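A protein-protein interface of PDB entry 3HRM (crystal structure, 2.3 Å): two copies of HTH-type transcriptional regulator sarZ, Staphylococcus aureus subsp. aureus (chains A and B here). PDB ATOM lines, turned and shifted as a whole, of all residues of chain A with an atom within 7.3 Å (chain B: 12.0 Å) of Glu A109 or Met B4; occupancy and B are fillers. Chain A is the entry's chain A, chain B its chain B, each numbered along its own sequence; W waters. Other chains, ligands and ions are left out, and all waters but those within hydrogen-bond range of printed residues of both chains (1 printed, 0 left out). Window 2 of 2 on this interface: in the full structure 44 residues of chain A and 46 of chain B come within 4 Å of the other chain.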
ATOM      1  N   TYR A  32      16.612  16.902  -8.642  1.00  0.00           N
ATOM      2  CA  TYR A  32      16.496  18.204  -8.014  1.00  0.00           C
ATOM      3  C   TYR A  32      17.432  18.275  -6.832  1.00  0.00           C
ATOM      4  O   TYR A  32      17.455  19.266  -6.114  1.00  0.00           O
ATOM      5  CB  TYR A  32      15.073  18.444  -7.534  1.00  0.00           C
ATOM      6  CG  TYR A  32      14.076  18.622  -8.645  1.00  0.00           C
ATOM      7  CD1 TYR A  32      13.818  19.886  -9.175  1.00  0.00           C
ATOM      8  CD2 TYR A  32      13.392  17.526  -9.178  1.00  0.00           C
ATOM      9  CE1 TYR A  32      12.901  20.058 -10.208  1.00  0.00           C
ATOM     10  CE2 TYR A  32      12.474  17.689 -10.211  1.00  0.00           C
ATOM     11  CZ  TYR A  32      12.232  18.955 -10.720  1.00  0.00           C
ATOM     12  OH  TYR A  32      11.315  19.122 -11.738  1.00  0.00           O
ATOM     13  N   TYR A  39      11.783  17.264   0.536  1.00  0.00           N
ATOM     14  CA  TYR A  39      10.663  17.507  -0.354  1.00  0.00           C
ATOM     15  C   TYR A  39       9.415  17.737   0.499  1.00  0.00           C
ATOM     16  O   TYR A  39       8.638  18.663   0.252  1.00  0.00           O
ATOM     17  CB  TYR A  39      10.450  16.293  -1.259  1.00  0.00           C
ATOM     18  CG  TYR A  39       9.032  16.158  -1.763  1.00  0.00           C
ATOM     19  CD1 TYR A  39       8.549  17.003  -2.757  1.00  0.00           C
ATOM     20  CD2 TYR A  39       8.165  15.198  -1.224  1.00  0.00           C
ATOM     21  CE1 TYR A  39       7.245  16.903  -3.209  1.00  0.00           C
ATOM     22  CE2 TYR A  39       6.851  15.093  -1.668  1.00  0.00           C
ATOM     23  CZ  TYR A  39       6.404  15.956  -2.663  1.00  0.00           C
ATOM     24  OH  TYR A  39       5.115  15.902  -3.110  1.00  0.00           O
ATOM     25  N   MET A  43       6.983  21.248   0.815  1.00  0.00           N
ATOM     26  CA  MET A  43       5.562  21.261   0.479  1.00  0.00           C
ATOM     27  C   MET A  43       4.731  21.591   1.717  1.00  0.00           C
ATOM     28  O   MET A  43       3.628  22.130   1.609  1.00  0.00           O
ATOM     29  CB  MET A  43       5.129  19.901  -0.080  1.00  0.00           C
ATOM     30  CG  MET A  43       5.873  19.458  -1.332  1.00  0.00           C
ATOM     31  SD  MET A  43       5.610  20.625  -2.851  1.00  0.00           S
ATOM     32  CE  MET A  43       4.002  19.836  -3.568  1.00  0.00           C
ATOM     33  N   ILE A 103      10.253  25.996  -7.097  1.00  0.00           N
ATOM     34  CA  ILE A 103      10.242  24.547  -7.280  1.00  0.00           C
ATOM     35  C   ILE A 103       8.992  23.847  -6.760  1.00  0.00           C
ATOM     36  O   ILE A 103       8.697  22.723  -7.163  1.00  0.00           O
ATOM     37  CB  ILE A 103      11.456  23.890  -6.605  1.00  0.00           C
ATOM     38  CG1 ILE A 103      11.507  24.313  -5.137  1.00  0.00           C
ATOM     39  CG2 ILE A 103      12.735  24.268  -7.340  1.00  0.00           C
ATOM     40  CD1 ILE A 103      12.551  23.590  -4.332  1.00  0.00           C
ATOM     41  N   LYS A 104       8.254  24.496  -5.867  1.00  0.00           N
ATOM     42  CA  LYS A 104       7.053  23.871  -5.325  1.00  0.00           C
ATOM     43  C   LYS A 104       6.040  23.491  -6.400  1.00  0.00           C
ATOM     44  O   LYS A 104       5.180  22.640  -6.169  1.00  0.00           O
ATOM     45  CB  LYS A 104       6.404  24.772  -4.270  1.00  0.00           C
ATOM     46  CG  LYS A 104       7.275  24.950  -3.033  1.00  0.00           C
ATOM     47  CD  LYS A 104       6.519  25.586  -1.877  1.00  0.00           C
ATOM     48  CE  LYS A 104       5.387  24.695  -1.404  1.00  0.00           C
ATOM     49  NZ  LYS A 104       4.729  25.236  -0.186  1.00  0.00           N
ATOM     50  N   SER A 105       6.146  24.109  -7.574  1.00  0.00           N
ATOM     51  CA  SER A 105       5.235  23.797  -8.671  1.00  0.00           C
ATOM     52  C   SER A 105       5.631  22.501  -9.388  1.00  0.00           C
ATOM     53  O   SER A 105       4.796  21.615  -9.567  1.00  0.00           O
ATOM     54  CB  SER A 105       5.160  24.969  -9.659  1.00  0.00           C
ATOM     55  OG  SER A 105       6.413  25.616  -9.788  1.00  0.00           O
ATOM     56  N   PRO A 106       6.905  22.376  -9.820  1.00  0.00           N
ATOM     57  CA  PRO A 106       7.314  21.141 -10.498  1.00  0.00           C
ATOM     58  C   PRO A 106       7.388  19.960  -9.527  1.00  0.00           C
ATOM     59  O   PRO A 106       7.223  18.803  -9.920  1.00  0.00           O
ATOM     60  CB  PRO A 106       8.682  21.499 -11.089  1.00  0.00           C
ATOM     61  CG  PRO A 106       9.203  22.544 -10.154  1.00  0.00           C
ATOM     62  CD  PRO A 106       7.976  23.387  -9.888  1.00  0.00           C
ATOM     63  N   LEU A 107       7.647  20.251  -8.255  1.00  0.00           N
ATOM     64  CA  LEU A 107       7.713  19.186  -7.266  1.00  0.00           C
ATOM     65  C   LEU A 107       6.304  18.643  -7.067  1.00  0.00           C
ATOM     66  O   LEU A 107       6.109  17.445  -6.875  1.00  0.00           O
ATOM     67  CB  LEU A 107       8.255  19.709  -5.939  1.00  0.00           C
ATOM     68  CG  LEU A 107       9.716  20.159  -5.904  1.00  0.00           C
ATOM     69  CD1 LEU A 107      10.013  20.699  -4.519  1.00  0.00           C
ATOM     70  CD2 LEU A 107      10.654  19.003  -6.245  1.00  0.00           C
ATOM     71  N   ALA A 108       5.326  19.541  -7.134  1.00  0.00           N
ATOM     72  CA  ALA A 108       3.927  19.182  -6.964  1.00  0.00           C
ATOM     73  C   ALA A 108       3.478  18.202  -8.037  1.00  0.00           C
ATOM     74  O   ALA A 108       2.517  17.459  -7.847  1.00  0.00           O
ATOM     75  CB  ALA A 108       3.060  20.435  -7.000  1.00  0.00           C
ATOM     76  N   GLU A 109       4.175  18.196  -9.166  1.00  0.00           N
ATOM     77  CA  GLU A 109       3.828  17.281 -10.243  1.00  0.00           C
ATOM     78  C   GLU A 109       4.368  15.870  -9.976  1.00  0.00           C
ATOM     79  O   GLU A 109       3.817  14.891 -10.472  1.00  0.00           O
ATOM     80  CB  GLU A 109       4.383  17.796 -11.575  1.00  0.00           C
ATOM     81  CG  GLU A 109       4.017  19.234 -11.897  1.00  0.00           C
ATOM     82  CD  GLU A 109       4.605  19.706 -13.219  1.00  0.00           C
ATOM     83  OE1 GLU A 109       5.806  19.454 -13.458  1.00  0.00           O
ATOM     84  OE2 GLU A 109       3.872  20.335 -14.012  1.00  0.00           O
ATOM     85  N   ILE A 110       5.434  15.763  -9.185  1.00  0.00           N
ATOM     86  CA  ILE A 110       6.037  14.461  -8.889  1.00  0.00           C
ATOM     87  C   ILE A 110       5.168  13.445  -8.136  1.00  0.00           C
ATOM     88  O   ILE A 110       5.207  12.256  -8.454  1.00  0.00           O
ATOM     89  CB  ILE A 110       7.355  14.610  -8.112  1.00  0.00           C
ATOM     90  CG1 ILE A 110       8.351  15.436  -8.931  1.00  0.00           C
ATOM     91  CG2 ILE A 110       7.939  13.234  -7.816  1.00  0.00           C
ATOM     92  CD1 ILE A 110       9.743  15.495  -8.326  1.00  0.00           C
ATOM     93  N   SER A 111       4.395  13.885  -7.148  1.00  0.00           N
ATOM     94  CA  SER A 111       3.558  12.943  -6.401  1.00  0.00           C
ATOM     95  C   SER A 111       2.568  12.231  -7.322  1.00  0.00           C
ATOM     96  O   SER A 111       2.318  11.032  -7.169  1.00  0.00           O
ATOM     97  CB  SER A 111       2.811  13.649  -5.262  1.00  0.00           C
ATOM     98  OG  SER A 111       1.932  14.633  -5.756  1.00  0.00           O
ATOM     99  N   VAL A 112       2.017  12.965  -8.285  1.00  0.00           N
ATOM    100  CA  VAL A 112       1.086  12.377  -9.239  1.00  0.00           C
ATOM    101  C   VAL A 112       1.756  11.193  -9.937  1.00  0.00           C
ATOM    102  O   VAL A 112       1.150  10.132 -10.113  1.00  0.00           O
ATOM    103  CB  VAL A 112       0.666  13.394 -10.314  1.00  0.00           C
ATOM    104  CG1 VAL A 112      -0.168  12.716 -11.377  1.00  0.00           C
ATOM    105  CG2 VAL A 112      -0.126  14.500  -9.685  1.00  0.00           C
ATOM    106  N   LYS A 113       3.013  11.382 -10.321  1.00  0.00           N
ATOM    107  CA  LYS A 113       3.768  10.338 -10.998  1.00  0.00           C
ATOM    108  C   LYS A 113       4.053   9.172 -10.081  1.00  0.00           C
ATOM    109  O   LYS A 113       3.879   8.026 -10.475  1.00  0.00           O
ATOM    110  CB  LYS A 113       5.096  10.882 -11.538  1.00  0.00           C
ATOM    111  CG  LYS A 113       4.940  11.888 -12.672  1.00  0.00           C
ATOM    112  CD  LYS A 113       6.292  12.404 -13.141  1.00  0.00           C
ATOM    113  CE  LYS A 113       6.156  13.257 -14.391  1.00  0.00           C
ATOM    114  NZ  LYS A 113       7.497  13.643 -14.902  1.00  0.00           N
ATOM    115  N   VAL A 114       4.496   9.458  -8.859  1.00  0.00           N
ATOM    116  CA  VAL A 114       4.807   8.386  -7.932  1.00  0.00           C
ATOM    117  C   VAL A 114       3.601   7.522  -7.635  1.00  0.00           C
ATOM    118  O   VAL A 114       3.697   6.301  -7.652  1.00  0.00           O
ATOM    119  CB  VAL A 114       5.365   8.913  -6.597  1.00  0.00           C
ATOM    120  CG1 VAL A 114       5.268   7.833  -5.534  1.00  0.00           C
ATOM    121  CG2 VAL A 114       6.821   9.318  -6.767  1.00  0.00           C
ATOM    122  N   ASN A 116       0.947   7.048  -9.437  1.00  0.00           N
ATOM    123  CA  ASN A 116       0.379   6.405 -10.620  1.00  0.00           C
ATOM    124  C   ASN A 116       1.075   5.064 -10.811  1.00  0.00           C
ATOM    125  O   ASN A 116       0.469   4.093 -11.255  1.00  0.00           O
ATOM    126  CB  ASN A 116       0.576   7.264 -11.871  1.00  0.00           C
ATOM    127  CG  ASN A 116      -0.387   8.425 -11.936  1.00  0.00           C
ATOM    128  OD1 ASN A 116      -1.575   8.266 -11.678  1.00  0.00           O
ATOM    129  ND2 ASN A 116       0.118   9.598 -12.298  1.00  0.00           N
ATOM    130  N   GLY B   1     -12.532  14.068  -8.234  1.00  0.00           N
ATOM    131  CA  GLY B   1     -11.128  14.134  -7.774  1.00  0.00           C
ATOM    132  C   GLY B   1     -10.099  13.915  -8.869  1.00  0.00           C
ATOM    133  O   GLY B   1     -10.015  12.828  -9.448  1.00  0.00           O
ATOM    134  N   SER B   2      -9.313  14.952  -9.160  1.00  0.00           N
ATOM    135  CA  SER B   2      -8.268  14.856 -10.174  1.00  0.00           C
ATOM    136  C   SER B   2      -7.144  14.034  -9.571  1.00  0.00           C
ATOM    137  O   SER B   2      -7.104  13.819  -8.357  1.00  0.00           O
ATOM    138  CB  SER B   2      -7.740  16.242 -10.545  1.00  0.00           C
ATOM    139  OG  SER B   2      -7.168  16.888  -9.421  1.00  0.00           O
ATOM    140  N   HIS B   3      -6.224  13.580 -10.409  1.00  0.00           N
ATOM    141  CA  HIS B   3      -5.138  12.770  -9.908  1.00  0.00           C
ATOM    142  C   HIS B   3      -4.174  13.568  -9.052  1.00  0.00           C
ATOM    143  O   HIS B   3      -3.496  13.014  -8.187  1.00  0.00           O
ATOM    144  CB  HIS B   3      -4.412  12.085 -11.065  1.00  0.00           C
ATOM    145  CG  HIS B   3      -5.218  10.996 -11.706  1.00  0.00           C
ATOM    146  ND1 HIS B   3      -4.674  10.065 -12.564  1.00  0.00           N
ATOM    147  CD2 HIS B   3      -6.536  10.700 -11.617  1.00  0.00           C
ATOM    148  CE1 HIS B   3      -5.622   9.241 -12.976  1.00  0.00           C
ATOM    149  NE2 HIS B   3      -6.760   9.605 -12.418  1.00  0.00           N
ATOM    150  N   MET B   4      -4.125  14.871  -9.288  1.00  0.00           N
ATOM    151  CA  MET B   4      -3.243  15.737  -8.525  1.00  0.00           C
ATOM    152  C   MET B   4      -3.719  15.781  -7.075  1.00  0.00           C
ATOM    153  O   MET B   4      -2.948  15.551  -6.150  1.00  0.00           O
ATOM    154  CB  MET B   4      -3.248  17.144  -9.127  1.00  0.00           C
ATOM    155  CG  MET B   4      -2.285  18.100  -8.462  1.00  0.00           C
ATOM    156  SD  MET B   4      -0.491  17.401  -8.513  1.00  0.00           S
ATOM    157  CE  MET B   4       0.069  18.161 -10.197  1.00  0.00           C
ATOM    158  N   TYR B   5      -5.003  16.069  -6.895  1.00  0.00           N
ATOM    159  CA  TYR B   5      -5.604  16.155  -5.565  1.00  0.00           C
ATOM    160  C   TYR B   5      -5.522  14.830  -4.824  1.00  0.00           C
ATOM    161  O   TYR B   5      -5.183  14.797  -3.648  1.00  0.00           O
ATOM    162  CB  TYR B   5      -7.069  16.581  -5.657  1.00  0.00           C
ATOM    163  CG  TYR B   5      -7.761  16.642  -4.306  1.00  0.00           C
ATOM    164  CD1 TYR B   5      -7.418  17.615  -3.371  1.00  0.00           C
ATOM    165  CD2 TYR B   5      -8.714  15.689  -3.947  1.00  0.00           C
ATOM    166  CE1 TYR B   5      -7.997  17.635  -2.113  1.00  0.00           C
ATOM    167  CE2 TYR B   5      -9.299  15.700  -2.692  1.00  0.00           C
ATOM    168  CZ  TYR B   5      -8.936  16.673  -1.780  1.00  0.00           C
ATOM    169  OH  TYR B   5      -9.506  16.660  -0.533  1.00  0.00           O
ATOM    170  N   LEU B   6      -5.837  13.743  -5.517  1.00  0.00           N
ATOM    171  CA  LEU B   6      -5.774  12.425  -4.911  1.00  0.00           C
ATOM    172  C   LEU B   6      -4.342  12.093  -4.501  1.00  0.00           C
ATOM    173  O   LEU B   6      -4.105  11.577  -3.408  1.00  0.00           O
ATOM    174  CB  LEU B   6      -6.285  11.370  -5.890  1.00  0.00           C
ATOM    175  CG  LEU B   6      -7.786  11.414  -6.164  1.00  0.00           C
ATOM    176  CD1 LEU B   6      -8.154  10.383  -7.239  1.00  0.00           C
ATOM    177  CD2 LEU B   6      -8.531  11.138  -4.870  1.00  0.00           C
ATOM    178  N   SER B   7      -3.389  12.398  -5.376  1.00  0.00           N
ATOM    179  CA  SER B   7      -1.993  12.115  -5.091  1.00  0.00           C
ATOM    180  C   SER B   7      -1.530  12.903  -3.880  1.00  0.00           C
ATOM    181  O   SER B   7      -0.779  12.399  -3.045  1.00  0.00           O
ATOM    182  CB  SER B   7      -1.129  12.465  -6.296  1.00  0.00           C
ATOM    183  OG  SER B   7      -1.453  11.620  -7.383  1.00  0.00           O
ATOM    184  N   LYS B   8      -1.989  14.144  -3.789  1.00  0.00           N
ATOM    185  CA  LYS B   8      -1.625  15.001  -2.677  1.00  0.00           C
ATOM    186  C   LYS B   8      -2.135  14.445  -1.343  1.00  0.00           C
ATOM    187  O   LYS B   8      -1.425  14.478  -0.345  1.00  0.00           O
ATOM    188  CB  LYS B   8      -2.175  16.409  -2.909  1.00  0.00           C
ATOM    189  CG  LYS B   8      -2.002  17.335  -1.722  1.00  0.00           C
ATOM    190  CD  LYS B   8      -2.392  18.768  -2.062  1.00  0.00           C
ATOM    191  CE  LYS B   8      -2.191  19.676  -0.853  1.00  0.00           C
ATOM    192  NZ  LYS B   8      -2.362  21.116  -1.197  1.00  0.00           N
ATOM    193  N   GLN B   9      -3.365  13.948  -1.331  1.00  0.00           N
ATOM    194  CA  GLN B   9      -3.958  13.392  -0.123  1.00  0.00           C
ATOM    195  C   GLN B   9      -3.254  12.100   0.280  1.00  0.00           C
ATOM    196  O   GLN B   9      -3.061  11.831   1.466  1.00  0.00           O
ATOM    197  CB  GLN B   9      -5.434  13.108  -0.354  1.00  0.00           C
ATOM    198  CG  GLN B   9      -6.263  14.350  -0.510  1.00  0.00           C
ATOM    199  CD  GLN B   9      -6.188  15.225   0.714  1.00  0.00           C
ATOM    200  OE1 GLN B   9      -5.830  16.394   0.627  1.00  0.00           O
ATOM    201  NE2 GLN B   9      -6.516  14.663   1.869  1.00  0.00           N
ATOM    202  N   LEU B  10      -2.889  11.299  -0.719  1.00  0.00           N
ATOM    203  CA  LEU B  10      -2.179  10.048  -0.483  1.00  0.00           C
ATOM    204  C   LEU B  10      -0.792  10.375   0.074  1.00  0.00           C
ATOM    205  O   LEU B  10      -0.330   9.751   1.028  1.00  0.00           O
ATOM    206  CB  LEU B  10      -2.044   9.252  -1.796  1.00  0.00           C
ATOM    207  CG  LEU B  10      -3.319   8.534  -2.257  1.00  0.00           C
ATOM    208  CD1 LEU B  10      -3.170   7.982  -3.670  1.00  0.00           C
ATOM    209  CD2 LEU B  10      -3.618   7.423  -1.278  1.00  0.00           C
ATOM    210  N   CSO B  11      -0.137  11.357  -0.533  1.00  0.00           N
ATOM    211  CA  CSO B  11       1.190  11.766  -0.100  1.00  0.00           C
ATOM    212  CB  CSO B  11       1.642  13.010  -0.881  1.00  0.00           C
ATOM    213  SG  CSO B  11       3.279  13.650  -0.368  1.00  0.00           S
ATOM    214  C   CSO B  11       1.148  12.083   1.394  1.00  0.00           C
ATOM    215  O   CSO B  11       1.858  11.473   2.211  1.00  0.00           O
ATOM    216  OD  CSO B  11       4.081  12.389  -0.638  1.00  0.00           O
ATOM    217  N   PHE B  12       0.292  13.034   1.737  1.00  0.00           N
ATOM    218  CA  PHE B  12       0.116  13.484   3.113  1.00  0.00           C
ATOM    219  C   PHE B  12      -0.304  12.375   4.092  1.00  0.00           C
ATOM    220  O   PHE B  12       0.335  12.173   5.128  1.00  0.00           O
ATOM    221  CB  PHE B  12      -0.926  14.619   3.131  1.00  0.00           C
ATOM    222  CG  PHE B  12      -1.222  15.181   4.506  1.00  0.00           C
ATOM    223  CD1 PHE B  12      -0.380  16.130   5.089  1.00  0.00           C
ATOM    224  CD2 PHE B  12      -2.356  14.764   5.214  1.00  0.00           C
ATOM    225  CE1 PHE B  12      -0.660  16.668   6.361  1.00  0.00           C
ATOM    226  CE2 PHE B  12      -2.656  15.290   6.491  1.00  0.00           C
ATOM    227  CZ  PHE B  12      -1.805  16.246   7.069  1.00  0.00           C
ATOM    228  N   LEU B  13      -1.379  11.658   3.769  1.00  0.00           N
ATOM    229  CA  LEU B  13      -1.888  10.632   4.669  1.00  0.00           C
ATOM    230  C   LEU B  13      -0.947   9.455   4.914  1.00  0.00           C
ATOM    231  O   LEU B  13      -0.878   8.949   6.028  1.00  0.00           O
ATOM    232  CB  LEU B  13      -3.266  10.167   4.193  1.00  0.00           C
ATOM    233  CG  LEU B  13      -4.330  11.280   4.342  1.00  0.00           C
ATOM    234  CD1 LEU B  13      -5.653  10.855   3.707  1.00  0.00           C
ATOM    235  CD2 LEU B  13      -4.532  11.604   5.815  1.00  0.00           C
ATOM    236  N   PHE B  14      -0.204   9.034   3.896  1.00  0.00           N
ATOM    237  CA  PHE B  14       0.746   7.940   4.072  1.00  0.00           C
ATOM    238  C   PHE B  14       1.910   8.439   4.936  1.00  0.00           C
ATOM    239  O   PHE B  14       2.404   7.738   5.821  1.00  0.00           O
ATOM    240  CB  PHE B  14       1.257   7.458   2.706  1.00  0.00           C
ATOM    241  CG  PHE B  14       0.512   6.266   2.168  1.00  0.00           C
ATOM    242  CD1 PHE B  14       0.594   5.032   2.818  1.00  0.00           C
ATOM    243  CD2 PHE B  14      -0.264   6.362   1.009  1.00  0.00           C
ATOM    244  CE1 PHE B  14      -0.091   3.892   2.317  1.00  0.00           C
ATOM    245  CE2 PHE B  14      -0.952   5.227   0.503  1.00  0.00           C
ATOM    246  CZ  PHE B  14      -0.857   3.995   1.167  1.00  0.00           C
HETATM  247  O   HOH W   1      -2.082   9.633  -9.473  1.00  0.00           O
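Of the 16 printed residues of chain A, 6 touch a printed residue of chain B. Hydrophobic or aromatic side chains of chain A within 4 Å of the printed part of chain B: Tyr A39 and Val A112. Along chain A the printed residues that touch a printed residue of chain B span positions 39 to 116. Of the 14 printed residues of chain B, 4 touch a printed residue of chain A. Printed residues of chain B that touch a printed residue of chain A: His B3, Met B4, Ser B7 and CSO B11. Among the printed residues, 8 pairs touch across the chains. Among the printed residues, no Asp or Glu carboxylate lies within 4 Å of a Lys or Arg side-chain nitrogen of the other chain.
No position is printed for both chains.
Among the printed residues, merely in contact across the chains: Val A112 with Met B4 (3.2 Å), Val A112 with Ser B7 (3.2 Å), Asn A116 with His B3 (3.7 Å), Ser A111 with Ser B7 (3.8 Å), Glu A109 with Met B4 (3.9 Å), Val A112 with His B3 (3.98 Å) and Tyr A39 with CSO B11 (3.995 Å).
SD of Met B4 sits close to O of Ala A108, 3.1 Å away.
The backbone carbonyl oxygen (O) of Val A112 is in hydrogen-bond range of the side-chain amide nitrogen (ND2) of Asn A116 (2.5 Å). OG of Ser B7 sits at hydrogen-bond distance from O of His B3, at 2.6 Å.
Printed residues of chain B within 4 Å of Tyr A39: CSO B11. No residue of chain B comes within 4 Å of Ser A105. No residue of chain B comes within 4 Å of Pro A106. Printed residues of chain B within 4 Å of Glu A109: Met B4. No residue of chain B comes within 4 Å of Ile A110. Of the printed residues of chain B, Asn A116 touches His B3. Of the printed residues of chain A, Met B4 touches Ala A108, Glu A109 and Val A112. Of the printed residues of chain A, Ser B7 touches Ser A111 and Val A112. The nearest printed residue of chain B that does not touch Glu A109 is Ser B7 (6.9 Å). The nearest printed residue of chain B that does not touch Val A112 is Tyr B5 (5.8 Å).
Water W1 lies within hydrogen-bond range of OD1 of Asn A116 (2.6 Å), OG of Ser B7 (3.0 Å) and O of Val A112 (3.3 Å).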
